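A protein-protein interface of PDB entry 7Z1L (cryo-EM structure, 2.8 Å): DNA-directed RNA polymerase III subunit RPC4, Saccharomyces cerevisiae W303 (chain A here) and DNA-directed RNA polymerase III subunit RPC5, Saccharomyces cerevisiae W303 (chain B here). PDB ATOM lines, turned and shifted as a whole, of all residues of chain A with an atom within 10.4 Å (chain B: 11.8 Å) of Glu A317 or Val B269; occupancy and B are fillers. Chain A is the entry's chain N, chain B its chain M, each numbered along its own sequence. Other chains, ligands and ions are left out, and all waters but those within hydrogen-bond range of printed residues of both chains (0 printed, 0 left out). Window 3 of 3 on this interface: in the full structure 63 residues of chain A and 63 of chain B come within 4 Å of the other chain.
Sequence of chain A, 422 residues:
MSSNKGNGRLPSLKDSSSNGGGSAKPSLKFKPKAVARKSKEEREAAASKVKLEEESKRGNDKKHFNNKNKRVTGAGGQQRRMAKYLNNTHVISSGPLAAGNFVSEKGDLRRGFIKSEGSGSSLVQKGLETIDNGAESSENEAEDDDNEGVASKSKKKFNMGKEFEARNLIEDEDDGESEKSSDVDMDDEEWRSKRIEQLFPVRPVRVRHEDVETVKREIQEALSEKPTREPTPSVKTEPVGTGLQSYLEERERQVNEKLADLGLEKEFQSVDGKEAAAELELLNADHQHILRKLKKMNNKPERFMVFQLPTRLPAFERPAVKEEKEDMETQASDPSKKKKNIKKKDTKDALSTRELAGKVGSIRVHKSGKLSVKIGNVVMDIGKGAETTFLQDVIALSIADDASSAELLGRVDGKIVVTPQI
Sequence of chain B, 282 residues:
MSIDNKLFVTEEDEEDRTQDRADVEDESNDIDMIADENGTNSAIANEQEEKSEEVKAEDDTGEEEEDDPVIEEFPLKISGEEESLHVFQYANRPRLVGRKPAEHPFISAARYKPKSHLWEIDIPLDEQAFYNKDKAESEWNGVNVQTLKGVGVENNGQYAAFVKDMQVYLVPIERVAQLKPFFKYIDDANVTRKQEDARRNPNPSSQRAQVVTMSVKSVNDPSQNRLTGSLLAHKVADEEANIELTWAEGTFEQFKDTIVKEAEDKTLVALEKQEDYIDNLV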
ATOM      1  N   LEU A 313     -19.549 -14.825  33.818  1.00  0.00           N
ATOM      2  CA  LEU A 313     -18.525 -15.318  32.919  1.00  0.00           C
ATOM      3  C   LEU A 313     -17.794 -14.146  32.268  1.00  0.00           C
ATOM      4  O   LEU A 313     -18.319 -13.031  32.217  1.00  0.00           O
ATOM      5  CB  LEU A 313     -19.153 -16.220  31.859  1.00  0.00           C
ATOM      6  CG  LEU A 313     -19.429 -17.645  32.335  1.00  0.00           C
ATOM      7  CD1 LEU A 313     -20.430 -18.338  31.430  1.00  0.00           C
ATOM      8  CD2 LEU A 313     -18.132 -18.429  32.405  1.00  0.00           C
ATOM      9  N   PRO A 314     -16.562 -14.362  31.802  1.00  0.00           N
ATOM     10  CA  PRO A 314     -15.844 -13.294  31.094  1.00  0.00           C
ATOM     11  C   PRO A 314     -16.597 -12.841  29.852  1.00  0.00           C
ATOM     12  O   PRO A 314     -17.244 -13.638  29.169  1.00  0.00           O
ATOM     13  CB  PRO A 314     -14.506 -13.946  30.734  1.00  0.00           C
ATOM     14  CG  PRO A 314     -14.322 -14.998  31.754  1.00  0.00           C
ATOM     15  CD  PRO A 314     -15.688 -15.515  32.083  1.00  0.00           C
ATOM     16  N   ALA A 315     -16.514 -11.541  29.574  1.00  0.00           N
ATOM     17  CA  ALA A 315     -17.277 -10.956  28.482  1.00  0.00           C
ATOM     18  C   ALA A 315     -16.781 -11.463  27.135  1.00  0.00           C
ATOM     19  O   ALA A 315     -15.577 -11.625  26.914  1.00  0.00           O
ATOM     20  CB  ALA A 315     -17.194  -9.431  28.532  1.00  0.00           C
ATOM     21  N   PHE A 316     -17.723 -11.714  26.232  1.00  0.00           N
ATOM     22  CA  PHE A 316     -17.431 -12.174  24.884  1.00  0.00           C
ATOM     23  C   PHE A 316     -17.991 -11.170  23.888  1.00  0.00           C
ATOM     24  O   PHE A 316     -19.034 -10.556  24.133  1.00  0.00           O
ATOM     25  CB  PHE A 316     -18.030 -13.561  24.633  1.00  0.00           C
ATOM     26  CG  PHE A 316     -17.221 -14.686  25.211  1.00  0.00           C
ATOM     27  CD1 PHE A 316     -16.061 -15.115  24.587  1.00  0.00           C
ATOM     28  CD2 PHE A 316     -17.618 -15.312  26.380  1.00  0.00           C
ATOM     29  CE1 PHE A 316     -15.315 -16.150  25.118  1.00  0.00           C
ATOM     30  CE2 PHE A 316     -16.876 -16.347  26.916  1.00  0.00           C
ATOM     31  CZ  PHE A 316     -15.724 -16.765  26.284  1.00  0.00           C
ATOM     32  N   GLU A 317     -17.286 -10.997  22.771  1.00  0.00           N
ATOM     33  CA  GLU A 317     -17.691 -10.016  21.773  1.00  0.00           C
ATOM     34  C   GLU A 317     -19.005 -10.423  21.116  1.00  0.00           C
ATOM     35  O   GLU A 317     -19.240 -11.602  20.836  1.00  0.00           O
ATOM     36  CB  GLU A 317     -16.596  -9.856  20.719  1.00  0.00           C
ATOM     37  CG  GLU A 317     -16.795  -8.674  19.784  1.00  0.00           C
ATOM     38  CD  GLU A 317     -15.611  -8.455  18.863  1.00  0.00           C
ATOM     39  OE1 GLU A 317     -14.648  -9.247  18.932  1.00  0.00           O
ATOM     40  OE2 GLU A 317     -15.644  -7.490  18.072  1.00  0.00           O
ATOM     41  N   ARG A 318     -19.866  -9.436  20.881  1.00  0.00           N
ATOM     42  CA  ARG A 318     -21.151  -9.691  20.254  1.00  0.00           C
ATOM     43  C   ARG A 318     -20.960 -10.132  18.803  1.00  0.00           C
ATOM     44  O   ARG A 318     -20.061  -9.646  18.111  1.00  0.00           O
ATOM     45  CB  ARG A 318     -22.028  -8.442  20.304  1.00  0.00           C
ATOM     46  CG  ARG A 318     -22.797  -8.270  21.604  1.00  0.00           C
ATOM     47  CD  ARG A 318     -23.228  -6.827  21.808  1.00  0.00           C
ATOM     48  NE  ARG A 318     -22.197  -6.035  22.468  1.00  0.00           N
ATOM     49  CZ  ARG A 318     -22.440  -5.037  23.307  1.00  0.00           C
ATOM     50  NH1 ARG A 318     -23.676  -4.684  23.621  1.00  0.00           N
ATOM     51  NH2 ARG A 318     -21.418  -4.380  23.847  1.00  0.00           N
ATOM     52  N   PRO A 319     -21.798 -11.060  18.314  1.00  0.00           N
ATOM     53  CA  PRO A 319     -21.694 -11.532  16.930  1.00  0.00           C
ATOM     54  C   PRO A 319     -22.279 -10.541  15.930  1.00  0.00           C
ATOM     55  O   PRO A 319     -21.936 -10.615  14.750  1.00  0.00           O
ATOM     56  CB  PRO A 319     -22.500 -12.841  16.933  1.00  0.00           C
ATOM     57  CG  PRO A 319     -22.936 -13.068  18.361  1.00  0.00           C
ATOM     58  CD  PRO A 319     -22.865 -11.752  19.052  1.00  0.00           C
ATOM     59  N   ALA A 350     -19.687  -7.417  27.054  1.00  0.00           N
ATOM     60  CA  ALA A 350     -20.582  -7.119  25.942  1.00  0.00           C
ATOM     61  C   ALA A 350     -21.867  -7.937  26.042  1.00  0.00           C
ATOM     62  O   ALA A 350     -22.913  -7.419  26.433  1.00  0.00           O
ATOM     63  CB  ALA A 350     -19.887  -7.381  24.618  1.00  0.00           C
ATOM     64  N   LEU A 351     -21.779  -9.214  25.680  1.00  0.00           N
ATOM     65  CA  LEU A 351     -22.935 -10.097  25.756  1.00  0.00           C
ATOM     66  C   LEU A 351     -23.281 -10.411  27.206  1.00  0.00           C
ATOM     67  O   LEU A 351     -22.401 -10.511  28.066  1.00  0.00           O
ATOM     68  CB  LEU A 351     -22.664 -11.391  24.991  1.00  0.00           C
ATOM     69  CG  LEU A 351     -23.146 -11.438  23.541  1.00  0.00           C
ATOM     70  CD1 LEU A 351     -22.844 -12.792  22.919  1.00  0.00           C
ATOM     71  CD2 LEU A 351     -24.631 -11.127  23.462  1.00  0.00           C
ATOM     72  N   SER A 352     -24.575 -10.563  27.474  1.00  0.00           N
ATOM     73  CA  SER A 352     -25.033 -10.912  28.809  1.00  0.00           C
ATOM     74  C   SER A 352     -24.639 -12.348  29.149  1.00  0.00           C
ATOM     75  O   SER A 352     -24.359 -13.167  28.270  1.00  0.00           O
ATOM     76  CB  SER A 352     -26.548 -10.741  28.919  1.00  0.00           C
ATOM     77  OG  SER A 352     -26.958  -9.495  28.385  1.00  0.00           O
ATOM     78  N   GLU A 355     -26.634 -14.958  27.673  1.00  0.00           N
ATOM     79  CA  GLU A 355     -26.673 -14.875  26.221  1.00  0.00           C
ATOM     80  C   GLU A 355     -25.528 -15.611  25.535  1.00  0.00           C
ATOM     81  O   GLU A 355     -25.452 -15.581  24.302  1.00  0.00           O
ATOM     82  CB  GLU A 355     -26.666 -13.408  25.778  1.00  0.00           C
ATOM     83  CG  GLU A 355     -28.047 -12.829  25.523  1.00  0.00           C
ATOM     84  CD  GLU A 355     -28.705 -13.408  24.285  1.00  0.00           C
ATOM     85  OE1 GLU A 355     -27.975 -13.783  23.343  1.00  0.00           O
ATOM     86  OE2 GLU A 355     -29.951 -13.489  24.255  1.00  0.00           O
ATOM     87  N   LEU A 356     -24.638 -16.258  26.286  1.00  0.00           N
ATOM     88  CA  LEU A 356     -23.556 -17.008  25.662  1.00  0.00           C
ATOM     89  C   LEU A 356     -24.091 -18.238  24.941  1.00  0.00           C
ATOM     90  O   LEU A 356     -25.024 -18.898  25.406  1.00  0.00           O
ATOM     91  CB  LEU A 356     -22.504 -17.434  26.692  1.00  0.00           C
ATOM     92  CG  LEU A 356     -21.468 -16.436  27.223  1.00  0.00           C
ATOM     93  CD1 LEU A 356     -22.062 -15.401  28.155  1.00  0.00           C
ATOM     94  CD2 LEU A 356     -20.332 -17.178  27.907  1.00  0.00           C
ATOM     95  N   ALA A 357     -23.490 -18.538  23.793  1.00  0.00           N
ATOM     96  CA  ALA A 357     -23.838 -19.716  23.016  1.00  0.00           C
ATOM     97  C   ALA A 357     -22.573 -20.255  22.366  1.00  0.00           C
ATOM     98  O   ALA A 357     -21.580 -19.542  22.214  1.00  0.00           O
ATOM     99  CB  ALA A 357     -24.900 -19.403  21.956  1.00  0.00           C
ATOM    100  N   GLY A 358     -22.617 -21.528  21.992  1.00  0.00           N
ATOM    101  CA  GLY A 358     -21.481 -22.129  21.329  1.00  0.00           C
ATOM    102  C   GLY A 358     -20.300 -22.359  22.260  1.00  0.00           C
ATOM    103  O   GLY A 358     -20.410 -22.345  23.486  1.00  0.00           O
ATOM    104  N   LYS A 359     -19.144 -22.573  21.634  1.00  0.00           N
ATOM    105  CA  LYS A 359     -17.929 -22.877  22.378  1.00  0.00           C
ATOM    106  C   LYS A 359     -17.431 -21.649  23.131  1.00  0.00           C
ATOM    107  O   LYS A 359     -17.349 -20.550  22.579  1.00  0.00           O
ATOM    108  CB  LYS A 359     -16.846 -23.385  21.424  1.00  0.00           C
ATOM    109  CG  LYS A 359     -15.446 -23.407  22.012  1.00  0.00           C
ATOM    110  CD  LYS A 359     -14.549 -24.378  21.266  1.00  0.00           C
ATOM    111  CE  LYS A 359     -13.109 -24.266  21.734  1.00  0.00           C
ATOM    112  NZ  LYS A 359     -12.366 -25.543  21.557  1.00  0.00           N
ATOM    113  N   VAL A 360     -17.099 -21.846  24.406  1.00  0.00           N
ATOM    114  CA  VAL A 360     -16.556 -20.770  25.230  1.00  0.00           C
ATOM    115  C   VAL A 360     -15.158 -21.057  25.749  1.00  0.00           C
ATOM    116  O   VAL A 360     -14.439 -20.112  26.121  1.00  0.00           O
ATOM    117  CB  VAL A 360     -17.503 -20.456  26.408  1.00  0.00           C
ATOM    118  CG1 VAL A 360     -18.846 -19.963  25.895  1.00  0.00           C
ATOM    119  CG2 VAL A 360     -17.676 -21.678  27.291  1.00  0.00           C
ATOM    120  N   GLY A 361     -14.715 -22.305  25.801  1.00  0.00           N
ATOM    121  CA  GLY A 361     -13.403 -22.592  26.341  1.00  0.00           C
ATOM    122  C   GLY A 361     -13.078 -24.062  26.239  1.00  0.00           C
ATOM    123  O   GLY A 361     -13.681 -24.794  25.454  1.00  0.00           O
ATOM    124  N   ILE A 375     -11.399 -20.326  29.990  1.00  0.00           N
ATOM    125  CA  ILE A 375     -12.552 -19.660  29.396  1.00  0.00           C
ATOM    126  C   ILE A 375     -12.094 -18.299  28.901  1.00  0.00           C
ATOM    127  O   ILE A 375     -11.518 -17.518  29.668  1.00  0.00           O
ATOM    128  CB  ILE A 375     -13.713 -19.520  30.398  1.00  0.00           C
ATOM    129  CG1 ILE A 375     -14.218 -20.896  30.833  1.00  0.00           C
ATOM    130  CG2 ILE A 375     -14.844 -18.711  29.793  1.00  0.00           C
ATOM    131  CD1 ILE A 375     -14.682 -21.766  29.693  1.00  0.00           C
ATOM    132  N   GLY A 376     -12.343 -18.021  27.628  1.00  0.00           N
ATOM    133  CA  GLY A 376     -11.884 -16.769  27.051  1.00  0.00           C
ATOM    134  C   GLY A 376     -10.370 -16.707  27.067  1.00  0.00           C
ATOM    135  O   GLY A 376      -9.686 -17.396  26.301  1.00  0.00           O
ATOM    136  N   ASN A 377      -9.832 -15.871  27.953  1.00  0.00           N
ATOM    137  CA  ASN A 377      -8.395 -15.761  28.157  1.00  0.00           C
ATOM    138  C   ASN A 377      -7.974 -16.047  29.593  1.00  0.00           C
ATOM    139  O   ASN A 377      -6.796 -15.873  29.922  1.00  0.00           O
ATOM    140  CB  ASN A 377      -7.903 -14.373  27.742  1.00  0.00           C
ATOM    141  CG  ASN A 377      -8.307 -14.009  26.332  1.00  0.00           C
ATOM    142  OD1 ASN A 377      -8.333 -14.862  25.446  1.00  0.00           O
ATOM    143  ND2 ASN A 377      -8.628 -12.739  26.114  1.00  0.00           N
ATOM    144  N   LEU B  76     -15.441 -26.874  25.512  1.00  0.00           N
ATOM    145  CA  LEU B  76     -16.579 -26.575  26.369  1.00  0.00           C
ATOM    146  C   LEU B  76     -17.546 -25.684  25.605  1.00  0.00           C
ATOM    147  O   LEU B  76     -17.170 -24.595  25.161  1.00  0.00           O
ATOM    148  CB  LEU B  76     -16.118 -25.877  27.651  1.00  0.00           C
ATOM    149  CG  LEU B  76     -16.923 -26.064  28.937  1.00  0.00           C
ATOM    150  CD1 LEU B  76     -16.780 -27.478  29.448  1.00  0.00           C
ATOM    151  CD2 LEU B  76     -16.476 -25.070  29.991  1.00  0.00           C
ATOM    152  N   ASP B 265     -22.787 -24.259  15.257  1.00  0.00           N
ATOM    153  CA  ASP B 265     -22.611 -23.274  14.197  1.00  0.00           C
ATOM    154  C   ASP B 265     -21.691 -22.127  14.601  1.00  0.00           C
ATOM    155  O   ASP B 265     -20.973 -21.589  13.751  1.00  0.00           O
ATOM    156  CB  ASP B 265     -23.971 -22.723  13.765  1.00  0.00           C
ATOM    157  CG  ASP B 265     -24.787 -22.196  14.933  1.00  0.00           C
ATOM    158  OD1 ASP B 265     -24.334 -22.319  16.090  1.00  0.00           O
ATOM    159  OD2 ASP B 265     -25.888 -21.657  14.691  1.00  0.00           O
ATOM    160  N   LYS B 266     -21.694 -21.739  15.873  1.00  0.00           N
ATOM    161  CA  LYS B 266     -21.055 -20.509  16.312  1.00  0.00           C
ATOM    162  C   LYS B 266     -19.824 -20.790  17.163  1.00  0.00           C
ATOM    163  O   LYS B 266     -19.781 -21.751  17.936  1.00  0.00           O
ATOM    164  CB  LYS B 266     -22.034 -19.641  17.108  1.00  0.00           C
ATOM    165  CG  LYS B 266     -23.036 -18.888  16.255  1.00  0.00           C
ATOM    166  CD  LYS B 266     -23.905 -17.977  17.106  1.00  0.00           C
ATOM    167  CE  LYS B 266     -24.821 -18.782  18.012  1.00  0.00           C
ATOM    168  NZ  LYS B 266     -25.722 -19.680  17.238  1.00  0.00           N
ATOM    169  N   THR B 267     -18.815 -19.935  16.999  1.00  0.00           N
ATOM    170  CA  THR B 267     -17.642 -19.898  17.863  1.00  0.00           C
ATOM    171  C   THR B 267     -17.414 -18.456  18.288  1.00  0.00           C
ATOM    172  O   THR B 267     -17.331 -17.563  17.439  1.00  0.00           O
ATOM    173  CB  THR B 267     -16.397 -20.447  17.155  1.00  0.00           C
ATOM    174  OG1 THR B 267     -16.262 -19.827  15.869  1.00  0.00           O
ATOM    175  CG2 THR B 267     -16.496 -21.956  16.981  1.00  0.00           C
ATOM    176  N   LEU B 268     -17.312 -18.232  19.595  1.00  0.00           N
ATOM    177  CA  LEU B 268     -17.201 -16.885  20.139  1.00  0.00           C
ATOM    178  C   LEU B 268     -15.746 -16.528  20.409  1.00  0.00           C
ATOM    179  O   LEU B 268     -14.978 -17.342  20.929  1.00  0.00           O
ATOM    180  CB  LEU B 268     -18.023 -16.751  21.422  1.00  0.00           C
ATOM    181  CG  LEU B 268     -19.450 -16.212  21.270  1.00  0.00           C
ATOM    182  CD1 LEU B 268     -20.324 -17.139  20.443  1.00  0.00           C
ATOM    183  CD2 LEU B 268     -20.074 -15.974  22.636  1.00  0.00           C
ATOM    184  N   VAL B 269     -15.377 -15.303  20.048  1.00  0.00           N
ATOM    185  CA  VAL B 269     -14.013 -14.817  20.215  1.00  0.00           C
ATOM    186  C   VAL B 269     -13.876 -14.171  21.588  1.00  0.00           C
ATOM    187  O   VAL B 269     -14.799 -13.507  22.076  1.00  0.00           O
ATOM    188  CB  VAL B 269     -13.634 -13.839  19.087  1.00  0.00           C
ATOM    189  CG1 VAL B 269     -13.683 -14.550  17.745  1.00  0.00           C
ATOM    190  CG2 VAL B 269     -14.563 -12.632  19.064  1.00  0.00           C
ATOM    191  N   ALA B 270     -12.736 -14.408  22.233  1.00  0.00           N
ATOM    192  CA  ALA B 270     -12.501 -13.866  23.563  1.00  0.00           C
ATOM    193  C   ALA B 270     -12.292 -12.359  23.503  1.00  0.00           C
ATOM    194  O   ALA B 270     -11.666 -11.835  22.577  1.00  0.00           O
ATOM    195  CB  ALA B 270     -11.288 -14.540  24.196  1.00  0.00           C
ATOM    196  N   LEU B 271     -12.824 -11.658  24.503  1.00  0.00           N
ATOM    197  CA  LEU B 271     -12.711 -10.207  24.586  1.00  0.00           C
ATOM    198  C   LEU B 271     -11.932  -9.757  25.815  1.00  0.00           C
ATOM    199  O   LEU B 271     -10.955  -9.013  25.690  1.00  0.00           O
ATOM    200  CB  LEU B 271     -14.109  -9.574  24.582  1.00  0.00           C
ATOM    201  CG  LEU B 271     -14.159  -8.061  24.798  1.00  0.00           C
ATOM    202  CD1 LEU B 271     -13.473  -7.334  23.653  1.00  0.00           C
ATOM    203  CD2 LEU B 271     -15.595  -7.588  24.956  1.00  0.00           C
ATOM    204  N   GLU B 272     -12.337 -10.194  27.005  1.00  0.00           N
ATOM    205  CA  GLU B 272     -11.756  -9.672  28.233  1.00  0.00           C
ATOM    206  C   GLU B 272     -10.367 -10.247  28.482  1.00  0.00           C
ATOM    207  O   GLU B 272     -10.093 -11.414  28.188  1.00  0.00           O
ATOM    208  CB  GLU B 272     -12.666  -9.980  29.421  1.00  0.00           C
ATOM    209  CG  GLU B 272     -12.575  -8.963  30.548  1.00  0.00           C
ATOM    210  CD  GLU B 272     -13.816  -8.944  31.417  1.00  0.00           C
ATOM    211  OE1 GLU B 272     -14.934  -8.950  30.861  1.00  0.00           O
ATOM    212  OE2 GLU B 272     -13.676  -8.919  32.657  1.00  0.00           O
ATOM    213  N   LYS B 273      -9.490  -9.411  29.030  1.00  0.00           N
ATOM    214  CA  LYS B 273      -8.159  -9.823  29.440  1.00  0.00           C
ATOM    215  C   LYS B 273      -8.253 -10.635  30.734  1.00  0.00           C
ATOM    216  O   LYS B 273      -9.237 -10.551  31.474  1.00  0.00           O
ATOM    217  CB  LYS B 273      -7.268  -8.583  29.607  1.00  0.00           C
ATOM    218  CG  LYS B 273      -5.816  -8.823  30.006  1.00  0.00           C
ATOM    219  CD  LYS B 273      -5.036  -9.482  28.879  1.00  0.00           C
ATOM    220  CE  LYS B 273      -3.566  -9.625  29.235  1.00  0.00           C
ATOM    221  NZ  LYS B 273      -2.802 -10.329  28.168  1.00  0.00           N
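The backbone carbonyl oxygen (O) of Leu B76 sits at hydrogen-bond distance from the backbone NH (N) of Val A360, at 2.9 Å.
The backbone carbonyl oxygen of Gly A361 is in hydrogen-bond range of the backbone NH of Leu B76, at 2.7 Å.
OE1 of Glu B272 sits close to N of Ala A315, at 3.3 Å.
The backbone carbonyl oxygen (O) of Glu B272 is in hydrogen-bond range of the side-chain amide nitrogen (ND2) of Asn A377, 2.9 Å away.
The backbone NH of Leu A351 lies within hydrogen-bond range of the backbone carbonyl oxygen of Phe A316 (3.4 Å).
O of Val A360 is in hydrogen-bond range of N of Gly A376 (3.3 Å).
The side-chain carboxylate (OD1) of Asp B265 is in salt-bridge range of the side-chain amino group (NZ) of Lys B266.
Phe A316 touches Leu B268.
Val B269 touches Phe A316 (O to CD1, 3.2 Å).
CD1 of Phe A316 touches CA of Ala B270 (3.9 Å).
Leu B271 touches Glu A317 (CB to N, 3.9 Å).
Ala A357 touches Leu B268.
N of Lys A359 touches O of Lys B266, at 3.8 Å.
Lys A359 touches Leu B268.
CD1 of Ile A375 touches CD2 of Leu B76, 3.8 Å away.
CA of Gly A376 touches CB of Ala B270, 3.7 Å away.
CB of Ala B270 touches OD1 of Asn A377, 3.2 Å away.
Glu A317 touches just these residues of chain B: Val B269 (3.4 Å) and Leu B271 (3.9 Å).
Of chain A, only Phe A316 and Glu A317 come within 4 Å of Val B269.
Ala A315 touches just these residues of chain B: Leu B271 (3.4 Å) and Glu B272 (3.3 Å).
No residue of chain B comes within 4 Å of Ala A350.
Gly A376 touches just one residue of chain B: Ala B270.
Leu B268 touches just these residues of chain A: Phe A316, Ala A357 and Lys A359.
Ala B270 touches three residues of chain A.
Of the printed residues of chain B, Lys A359 touches Leu B76 (3.4 Å), Lys B266 (3.8 Å) and Leu B268 (3.8 Å).
Of the printed residues of chain A, Glu B272 touches Ala A315 and Asn A377.
Printed residues of chain B within 4 Å of Ala A357: Lys B266 and Leu B268.
Asp B265 touches none of the printed residues of chain A.
Leu A313 touches none of the printed residues of chain B.
The nearest residue of chain A that does not touch Val B269 is Ala A315 (5.2 Å).
The nearest printed residue of chain B that does not touch Gly A358 is Leu B76 (4.3 Å).
Hydrophobic or aromatic side chains of chain A that line the printed part of chain B: Ala A315, Phe A316, Ala A357, Val A360 and Ile A375.
Of the 10 printed residues of chain B, 7 touch a printed residue of chain A.
Along chain B the printed residues that touch a printed residue of chain A span positions 76 to 272.
Among the printed residues, no Asp or Glu carboxylate lies within 4 Å of a Lys or Arg side-chain nitrogen of the other chain.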
